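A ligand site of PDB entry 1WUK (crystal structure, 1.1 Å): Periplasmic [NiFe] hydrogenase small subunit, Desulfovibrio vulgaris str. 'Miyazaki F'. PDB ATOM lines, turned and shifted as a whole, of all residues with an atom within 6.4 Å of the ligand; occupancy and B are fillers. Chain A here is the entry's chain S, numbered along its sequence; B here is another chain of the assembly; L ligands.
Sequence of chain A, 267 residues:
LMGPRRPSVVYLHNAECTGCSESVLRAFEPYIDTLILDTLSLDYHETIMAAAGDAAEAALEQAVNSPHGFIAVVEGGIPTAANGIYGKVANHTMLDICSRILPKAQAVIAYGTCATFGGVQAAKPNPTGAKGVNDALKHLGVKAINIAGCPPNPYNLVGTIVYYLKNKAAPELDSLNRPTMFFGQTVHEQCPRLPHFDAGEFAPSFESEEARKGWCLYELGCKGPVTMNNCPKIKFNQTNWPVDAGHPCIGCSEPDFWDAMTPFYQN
N of Cys 20 is in hydrogen-bond range of OE1 of Glu 75 (3.1 Å). SG of Cys 17 lies close to N of Gly 19. SG of Cys 114 lies close to NE2 of Gln 121, 3.3 Å away. O of Cys 150 is in hydrogen-bond range of NH2 of Arg 61 of chain B (2.9 Å). O of Gly 149 sits at hydrogen-bond distance from N of Thr 113, 2.9 Å away. The backbone carbonyl oxygen (O) of Arg 61 of chain B sits at hydrogen-bond distance from the guanidinium group (NH1) of Arg 41 of chain B (2.8 Å). OG1 of Thr 18 sits at hydrogen-bond distance from OE1 of Glu 16, at 2.7 Å. OE1 of Glu 75 lies close to N of Thr 18, at 3.4 Å.
An iron atom (FE4) of the ligand is bound by the side-chain sulfur (SG) of Cys 20. A sulfur (S3) of the ligand lies close to the backbone NH of Cys 17, at 3.5 Å. An iron atom (FE1) of the ligand is bound by the side-chain sulfur (SG) of Cys 17. S1 of the ligand lies close to N of Cys 114 (3.5 Å). SG of Cys 114 is bound to FE2 of the ligand (2.3 Å). An iron atom (FE3) of the ligand is bound by the side-chain sulfur (SG) of Cys 150 (2.3 Å). The backbone NH (N) of Thr 113 lies close to a sulfur (S1) of the ligand. A sulfur (S2) of the ligand sits close to a ring nitrogen (ND1) of His 217 of chain B.
The backbone carbonyl oxygen (O) of Gly 149 sits close to a sulfur (S1) of the ligand (3.6 Å). The backbone nitrogen of Pro 151 sits close to a sulfur (S2) of the ligand, 3.6 Å away. Merely in contact with the ligand: Glu 16 (3.6 Å), Gly 19 (3.9 Å), Glu 75 (3.9 Å), Gly 112 (3.8 Å) and Arg 61 of chain B (3.4 Å). Hydrophobic or aromatic side chains that line the ligand: Pro 151 and His 217 of chain B. Of the 29 residues printed, 13 come within 4 Å of the ligand. The nearest printed residue that does not touch the ligand is Val 120 (4.002 Å).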
ATOM      1  N   ALA A  15      -2.470  -5.556  26.361  1.00  0.00           N
ATOM      2  CA  ALA A  15      -3.501  -6.379  25.718  1.00  0.00           C
ATOM      3  C   ALA A  15      -2.802  -7.629  25.229  1.00  0.00           C
ATOM      4  O   ALA A  15      -2.099  -7.610  24.213  1.00  0.00           O
ATOM      5  CB  ALA A  15      -4.166  -5.604  24.603  1.00  0.00           C
ATOM      6  N   GLU A  16      -2.980  -8.693  25.977  1.00  0.00           N
ATOM      7  CA  GLU A  16      -2.160  -9.897  25.864  1.00  0.00           C
ATOM      8  C   GLU A  16      -2.972 -11.094  26.344  1.00  0.00           C
ATOM      9  O   GLU A  16      -3.990 -10.945  27.010  1.00  0.00           O
ATOM     10  CB  GLU A  16      -0.834  -9.769  26.588  1.00  0.00           C
ATOM     11  CG  GLU A  16      -0.851  -9.216  27.974  1.00  0.00           C
ATOM     12  CD  GLU A  16      -1.326 -10.075  29.044  1.00  0.00           C
ATOM     13  OE1 GLU A  16      -0.903 -11.262  29.033  1.00  0.00           O
ATOM     14  OE2 GLU A  16      -2.059  -9.598  29.965  1.00  0.00           O
ATOM     15  N   CYS A  17      -2.471 -12.268  26.002  1.00  0.00           N
ATOM     16  CA  CYS A  17      -3.106 -13.527  26.372  1.00  0.00           C
ATOM     17  C   CYS A  17      -2.319 -14.296  27.450  1.00  0.00           C
ATOM     18  O   CYS A  17      -2.746 -15.382  27.850  1.00  0.00           O
ATOM     19  CB  CYS A  17      -3.287 -14.424  25.150  1.00  0.00           C
ATOM     20  SG  CYS A  17      -1.806 -15.328  24.593  1.00  0.00           S
ATOM     21  N   THR A  18      -1.160 -13.766  27.853  1.00  0.00           N
ATOM     22  CA  THR A  18      -0.227 -14.331  28.808  1.00  0.00           C
ATOM     23  C   THR A  18       0.541 -15.513  28.240  1.00  0.00           C
ATOM     24  O   THR A  18       1.385 -16.124  28.929  1.00  0.00           O
ATOM     25  CB  THR A  18      -0.941 -14.590  30.179  1.00  0.00           C
ATOM     26  OG1 THR A  18      -1.645 -13.397  30.498  1.00  0.00           O
ATOM     27  CG2 THR A  18      -0.023 -14.955  31.316  1.00  0.00           C
ATOM     28  N   GLY A  19       0.383 -15.806  26.966  1.00  0.00           N
ATOM     29  CA  GLY A  19       1.200 -16.827  26.334  1.00  0.00           C
ATOM     30  C   GLY A  19       2.651 -16.460  26.255  1.00  0.00           C
ATOM     31  O   GLY A  19       3.520 -17.333  26.298  1.00  0.00           O
ATOM     32  N   CYS A  20       2.964 -15.161  26.120  1.00  0.00           N
ATOM     33  CA  CYS A  20       4.336 -14.756  26.150  1.00  0.00           C
ATOM     34  C   CYS A  20       4.949 -14.983  27.536  1.00  0.00           C
ATOM     35  O   CYS A  20       6.042 -15.515  27.650  1.00  0.00           O
ATOM     36  CB  CYS A  20       4.474 -13.321  25.637  1.00  0.00           C
ATOM     37  SG  CYS A  20       4.242 -13.163  23.845  1.00  0.00           S
ATOM     38  N   SER A  21       4.251 -14.628  28.596  1.00  0.00           N
ATOM     39  CA  SER A  21       4.758 -14.929  29.947  1.00  0.00           C
ATOM     40  C   SER A  21       4.949 -16.436  30.120  1.00  0.00           C
ATOM     41  O   SER A  21       5.953 -16.858  30.691  1.00  0.00           O
ATOM     42  CB  SER A  21       3.785 -14.437  31.030  1.00  0.00           C
ATOM     43  OG  SER A  21       3.834 -13.072  31.240  1.00  0.00           O
ATOM     44  N   GLU A  75       4.750  -7.145  27.355  1.00  0.00           N
ATOM     45  CA  GLU A  75       3.921  -8.135  26.694  1.00  0.00           C
ATOM     46  C   GLU A  75       2.589  -7.495  26.353  1.00  0.00           C
ATOM     47  O   GLU A  75       1.976  -6.856  27.220  1.00  0.00           O
ATOM     48  CB  GLU A  75       3.722  -9.367  27.627  1.00  0.00           C
ATOM     49  CG  GLU A  75       2.799 -10.455  27.149  1.00  0.00           C
ATOM     50  CD  GLU A  75       2.758 -11.693  28.043  1.00  0.00           C
ATOM     51  OE1 GLU A  75       2.058 -12.670  27.703  1.00  0.00           O
ATOM     52  OE2 GLU A  75       3.476 -11.630  29.063  1.00  0.00           O
ATOM     53  N   GLY A  76       2.111  -7.670  25.144  1.00  0.00           N
ATOM     54  CA  GLY A  76       0.824  -7.159  24.739  1.00  0.00           C
ATOM     55  C   GLY A  76       0.873  -5.856  23.951  1.00  0.00           C
ATOM     56  O   GLY A  76       1.765  -5.024  24.125  1.00  0.00           O
ATOM     57  N   GLY A  77      -0.139  -5.672  23.104  1.00  0.00           N
ATOM     58  CA  GLY A  77      -0.322  -4.436  22.395  1.00  0.00           C
ATOM     59  C   GLY A  77      -0.948  -3.371  23.296  1.00  0.00           C
ATOM     60  O   GLY A  77      -1.545  -3.684  24.327  1.00  0.00           O
ATOM     61  N   TYR A 111       8.183  -8.001  23.840  1.00  0.00           N
ATOM     62  CA  TYR A 111       8.253  -9.454  23.781  1.00  0.00           C
ATOM     63  C   TYR A 111       6.904  -9.964  23.290  1.00  0.00           C
ATOM     64  O   TYR A 111       5.888  -9.802  23.974  1.00  0.00           O
ATOM     65  CB  TYR A 111       8.642 -10.036  25.147  1.00  0.00           C
ATOM     66  CG  TYR A 111       8.876 -11.539  25.076  1.00  0.00           C
ATOM     67  CD1 TYR A 111       9.864 -12.077  24.267  1.00  0.00           C
ATOM     68  CD2 TYR A 111       8.096 -12.401  25.823  1.00  0.00           C
ATOM     69  CE1 TYR A 111      10.077 -13.450  24.208  1.00  0.00           C
ATOM     70  CE2 TYR A 111       8.312 -13.781  25.769  1.00  0.00           C
ATOM     71  CZ  TYR A 111       9.286 -14.304  24.938  1.00  0.00           C
ATOM     72  OH  TYR A 111       9.540 -15.650  24.833  1.00  0.00           O
ATOM     73  N   GLY A 112       6.917 -10.574  22.104  1.00  0.00           N
ATOM     74  CA  GLY A 112       5.788 -11.139  21.409  1.00  0.00           C
ATOM     75  C   GLY A 112       5.225 -10.197  20.350  1.00  0.00           C
ATOM     76  O   GLY A 112       5.316  -8.988  20.460  1.00  0.00           O
ATOM     77  N   THR A 113       4.652 -10.805  19.317  1.00  0.00           N
ATOM     78  CA  THR A 113       4.107 -10.069  18.198  1.00  0.00           C
ATOM     79  C   THR A 113       3.089  -9.023  18.611  1.00  0.00           C
ATOM     80  O   THR A 113       3.013  -7.982  17.943  1.00  0.00           O
ATOM     81  CB  THR A 113       3.517 -11.073  17.189  1.00  0.00           C
ATOM     82  OG1 THR A 113       4.619 -11.767  16.661  1.00  0.00           O
ATOM     83  CG2 THR A 113       2.781 -10.397  16.020  1.00  0.00           C
ATOM     84  N   CYS A 114       2.322  -9.222  19.656  1.00  0.00           N
ATOM     85  CA  CYS A 114       1.406  -8.158  20.119  1.00  0.00           C
ATOM     86  C   CYS A 114       2.202  -6.902  20.548  1.00  0.00           C
ATOM     87  O   CYS A 114       1.875  -5.790  20.092  1.00  0.00           O
ATOM     88  CB  CYS A 114       0.546  -8.610  21.278  1.00  0.00           C
ATOM     89  SG  CYS A 114      -0.621  -9.942  20.860  1.00  0.00           S
ATOM     90  N   ALA A 115       3.187  -7.062  21.408  1.00  0.00           N
ATOM     91  CA  ALA A 115       3.966  -5.917  21.822  1.00  0.00           C
ATOM     92  C   ALA A 115       4.807  -5.358  20.697  1.00  0.00           C
ATOM     93  O   ALA A 115       5.034  -4.126  20.637  1.00  0.00           O
ATOM     94  CB  ALA A 115       4.860  -6.280  22.994  1.00  0.00           C
ATOM     95  N   GLY A 119      -0.341  -7.314  17.021  1.00  0.00           N
ATOM     96  CA  GLY A 119      -0.849  -8.629  17.265  1.00  0.00           C
ATOM     97  C   GLY A 119      -2.304  -8.842  17.060  1.00  0.00           C
ATOM     98  O   GLY A 119      -2.985  -8.179  16.299  1.00  0.00           O
ATOM     99  N   VAL A 120      -2.849  -9.872  17.749  1.00  0.00           N
ATOM    100  CA  VAL A 120      -4.147 -10.421  17.412  1.00  0.00           C
ATOM    101  C   VAL A 120      -5.247  -9.386  17.566  1.00  0.00           C
ATOM    102  O   VAL A 120      -6.139  -9.291  16.719  1.00  0.00           O
ATOM    103  CB  VAL A 120      -4.417 -11.706  18.205  1.00  0.00           C
ATOM    104  CG1 VAL A 120      -4.577 -11.479  19.709  1.00  0.00           C
ATOM    105  CG2 VAL A 120      -5.586 -12.484  17.624  1.00  0.00           C
ATOM    106  N   GLN A 121      -5.222  -8.576  18.621  1.00  0.00           N
ATOM    107  CA  GLN A 121      -6.262  -7.569  18.807  1.00  0.00           C
ATOM    108  C   GLN A 121      -6.133  -6.420  17.804  1.00  0.00           C
ATOM    109  O   GLN A 121      -7.092  -5.656  17.649  1.00  0.00           O
ATOM    110  CB  GLN A 121      -6.284  -7.053  20.256  1.00  0.00           C
ATOM    111  CG  GLN A 121      -5.001  -6.468  20.786  1.00  0.00           C
ATOM    112  CD  GLN A 121      -4.083  -7.506  21.341  1.00  0.00           C
ATOM    113  OE1 GLN A 121      -4.523  -8.377  22.091  1.00  0.00           O
ATOM    114  NE2 GLN A 121      -2.811  -7.511  20.986  1.00  0.00           N
ATOM    115  N   GLY A 149       7.101 -13.259  17.519  1.00  0.00           N
ATOM    116  CA  GLY A 149       6.487 -14.550  17.569  1.00  0.00           C
ATOM    117  C   GLY A 149       5.273 -14.578  18.505  1.00  0.00           C
ATOM    118  O   GLY A 149       5.101 -13.700  19.341  1.00  0.00           O
ATOM    119  N   CYS A 150       4.449 -15.623  18.356  1.00  0.00           N
ATOM    120  CA  CYS A 150       3.161 -15.665  19.044  1.00  0.00           C
ATOM    121  C   CYS A 150       2.931 -17.020  19.713  1.00  0.00           C
ATOM    122  O   CYS A 150       2.068 -17.816  19.291  1.00  0.00           O
ATOM    123  CB  CYS A 150       2.054 -15.296  18.039  1.00  0.00           C
ATOM    124  SG  CYS A 150       0.429 -14.919  18.747  1.00  0.00           S
ATOM    125  N   PRO A 151       3.669 -17.316  20.787  1.00  0.00           N
ATOM    126  CA  PRO A 151       4.714 -16.471  21.396  1.00  0.00           C
ATOM    127  C   PRO A 151       6.077 -16.722  20.764  1.00  0.00           C
ATOM    128  O   PRO A 151       6.288 -17.700  20.021  1.00  0.00           O
ATOM    129  CB  PRO A 151       4.695 -16.915  22.842  1.00  0.00           C
ATOM    130  CG  PRO A 151       4.368 -18.388  22.739  1.00  0.00           C
ATOM    131  CD  PRO A 151       3.385 -18.501  21.602  1.00  0.00           C
ATOM    132  N   PRO A 152       7.033 -15.858  21.070  1.00  0.00           N
ATOM    133  CA  PRO A 152       8.404 -16.075  20.647  1.00  0.00           C
ATOM    134  C   PRO A 152       9.013 -17.304  21.306  1.00  0.00           C
ATOM    135  O   PRO A 152       8.521 -17.810  22.292  1.00  0.00           O
ATOM    136  CB  PRO A 152       9.148 -14.822  21.107  1.00  0.00           C
ATOM    137  CG  PRO A 152       8.078 -13.801  21.352  1.00  0.00           C
ATOM    138  CD  PRO A 152       6.942 -14.652  21.889  1.00  0.00           C
ATOM    139  N   TRP A 258      -1.899 -11.699  11.047  1.00  0.00           N
ATOM    140  CA  TRP A 258      -3.269 -12.107  11.105  1.00  0.00           C
ATOM    141  C   TRP A 258      -4.047 -11.693   9.834  1.00  0.00           C
ATOM    142  O   TRP A 258      -4.989 -12.355   9.414  1.00  0.00           O
ATOM    143  CB  TRP A 258      -3.948 -11.476  12.337  1.00  0.00           C
ATOM    144  CG  TRP A 258      -3.293 -11.943  13.597  1.00  0.00           C
ATOM    145  CD1 TRP A 258      -2.420 -11.246  14.390  1.00  0.00           C
ATOM    146  CD2 TRP A 258      -3.453 -13.230  14.203  1.00  0.00           C
ATOM    147  NE1 TRP A 258      -2.034 -12.009  15.465  1.00  0.00           N
ATOM    148  CE2 TRP A 258      -2.646 -13.223  15.345  1.00  0.00           C
ATOM    149  CE3 TRP A 258      -4.171 -14.370  13.868  1.00  0.00           C
ATOM    150  CZ2 TRP A 258      -2.560 -14.349  16.200  1.00  0.00           C
ATOM    151  CZ3 TRP A 258      -4.057 -15.455  14.690  1.00  0.00           C
ATOM    152  CH2 TRP A 258      -3.256 -15.468  15.826  1.00  0.00           C
ATOM    153  N   ARG B  41     -10.451  -7.093  24.146  1.00  0.00           N
ATOM    154  CA  ARG B  41      -9.749  -7.240  22.858  1.00  0.00           C
ATOM    155  C   ARG B  41     -10.692  -7.341  21.674  1.00  0.00           C
ATOM    156  O   ARG B  41     -10.415  -6.778  20.615  1.00  0.00           O
ATOM    157  CB  ARG B  41      -8.770  -8.450  22.907  1.00  0.00           C
ATOM    158  CG  ARG B  41      -7.588  -8.195  23.796  1.00  0.00           C
ATOM    159  CD  ARG B  41      -6.643  -9.379  23.998  1.00  0.00           C
ATOM    160  NE  ARG B  41      -7.384 -10.441  24.679  1.00  0.00           N
ATOM    161  CZ  ARG B  41      -7.164 -11.748  24.558  1.00  0.00           C
ATOM    162  NH1 ARG B  41      -6.115 -12.212  23.890  1.00  0.00           N
ATOM    163  NH2 ARG B  41      -8.024 -12.590  25.129  1.00  0.00           N
ATOM    164  N   ARG B  61      -5.420 -17.644  20.721  1.00  0.00           N
ATOM    165  CA  ARG B  61      -4.846 -16.460  21.344  1.00  0.00           C
ATOM    166  C   ARG B  61      -5.812 -15.751  22.286  1.00  0.00           C
ATOM    167  O   ARG B  61      -5.454 -14.724  22.850  1.00  0.00           O
ATOM    168  CB  ARG B  61      -4.247 -15.516  20.333  1.00  0.00           C
ATOM    169  CG  ARG B  61      -2.896 -15.924  19.764  1.00  0.00           C
ATOM    170  CD  ARG B  61      -2.902 -17.240  19.058  1.00  0.00           C
ATOM    171  NE  ARG B  61      -1.562 -17.491  18.479  1.00  0.00           N
ATOM    172  CZ  ARG B  61      -1.231 -18.575  17.821  1.00  0.00           C
ATOM    173  NH1 ARG B  61      -2.179 -19.406  17.389  1.00  0.00           N
ATOM    174  NH2 ARG B  61       0.029 -18.802  17.550  1.00  0.00           N
ATOM    175  N   CYS B  63      -6.090 -17.095  25.042  1.00  0.00           N
ATOM    176  CA  CYS B  63      -5.397 -17.359  26.304  1.00  0.00           C
ATOM    177  C   CYS B  63      -4.217 -18.299  26.099  1.00  0.00           C
ATOM    178  O   CYS B  63      -4.374 -19.342  25.472  1.00  0.00           O
ATOM    179  CB  CYS B  63      -6.362 -17.973  27.285  1.00  0.00           C
ATOM    180  SG  CYS B  63      -5.612 -18.122  28.949  1.00  0.00           S
ATOM    181  N   GLY B  64      -3.098 -17.900  26.660  1.00  0.00           N
ATOM    182  CA  GLY B  64      -1.873 -18.716  26.639  1.00  0.00           C
ATOM    183  C   GLY B  64      -1.602 -19.497  27.896  1.00  0.00           C
ATOM    184  O   GLY B  64      -0.634 -20.250  27.912  1.00  0.00           O
ATOM    185  N   PRO B 216       3.934 -22.530  24.521  1.00  0.00           N
ATOM    186  CA  PRO B 216       2.495 -22.310  24.287  1.00  0.00           C
ATOM    187  C   PRO B 216       2.118 -22.272  22.812  1.00  0.00           C
ATOM    188  O   PRO B 216       2.921 -22.030  21.895  1.00  0.00           O
ATOM    189  CB  PRO B 216       2.258 -20.943  24.931  1.00  0.00           C
ATOM    190  CG  PRO B 216       3.382 -20.714  25.878  1.00  0.00           C
ATOM    191  CD  PRO B 216       4.544 -21.372  25.194  1.00  0.00           C
ATOM    192  N   HIS B 217       0.858 -22.452  22.598  1.00  0.00           N
ATOM    193  CA  HIS B 217       0.045 -22.329  21.386  1.00  0.00           C
ATOM    194  C   HIS B 217       0.402 -23.438  20.414  1.00  0.00           C
ATOM    195  O   HIS B 217       1.254 -23.352  19.542  1.00  0.00           O
ATOM    196  CB  HIS B 217       0.133 -20.922  20.793  1.00  0.00           C
ATOM    197  CG  HIS B 217      -0.558 -19.884  21.625  1.00  0.00           C
ATOM    198  ND1 HIS B 217      -0.402 -18.549  21.628  1.00  0.00           N
ATOM    199  CD2 HIS B 217      -1.555 -20.195  22.556  1.00  0.00           C
ATOM    200  CE1 HIS B 217      -1.304 -18.028  22.520  1.00  0.00           C
ATOM    201  NE2 HIS B 217      -1.977 -19.020  23.069  1.00  0.00           N
HETATM  202 FE1  LIG L   1      -0.506 -14.000  23.302  1.00  0.00          FE
HETATM  203 FE2  LIG L   1       0.191 -11.765  21.953  1.00  0.00          FE
HETATM  204 FE3  LIG L   1       0.673 -14.147  20.881  1.00  0.00          FE
HETATM  205 FE4  LIG L   1       2.139 -13.348  23.074  1.00  0.00          FE
HETATM  206  S1  LIG L   1       2.199 -12.416  21.011  1.00  0.00           S
HETATM  207  S2  LIG L   1       1.205 -15.446  22.660  1.00  0.00           S
HETATM  208  S3  LIG L   1       0.519 -12.091  24.186  1.00  0.00           S
HETATM  209  S4  LIG L   1      -1.435 -13.287  21.405  1.00  0.00           S
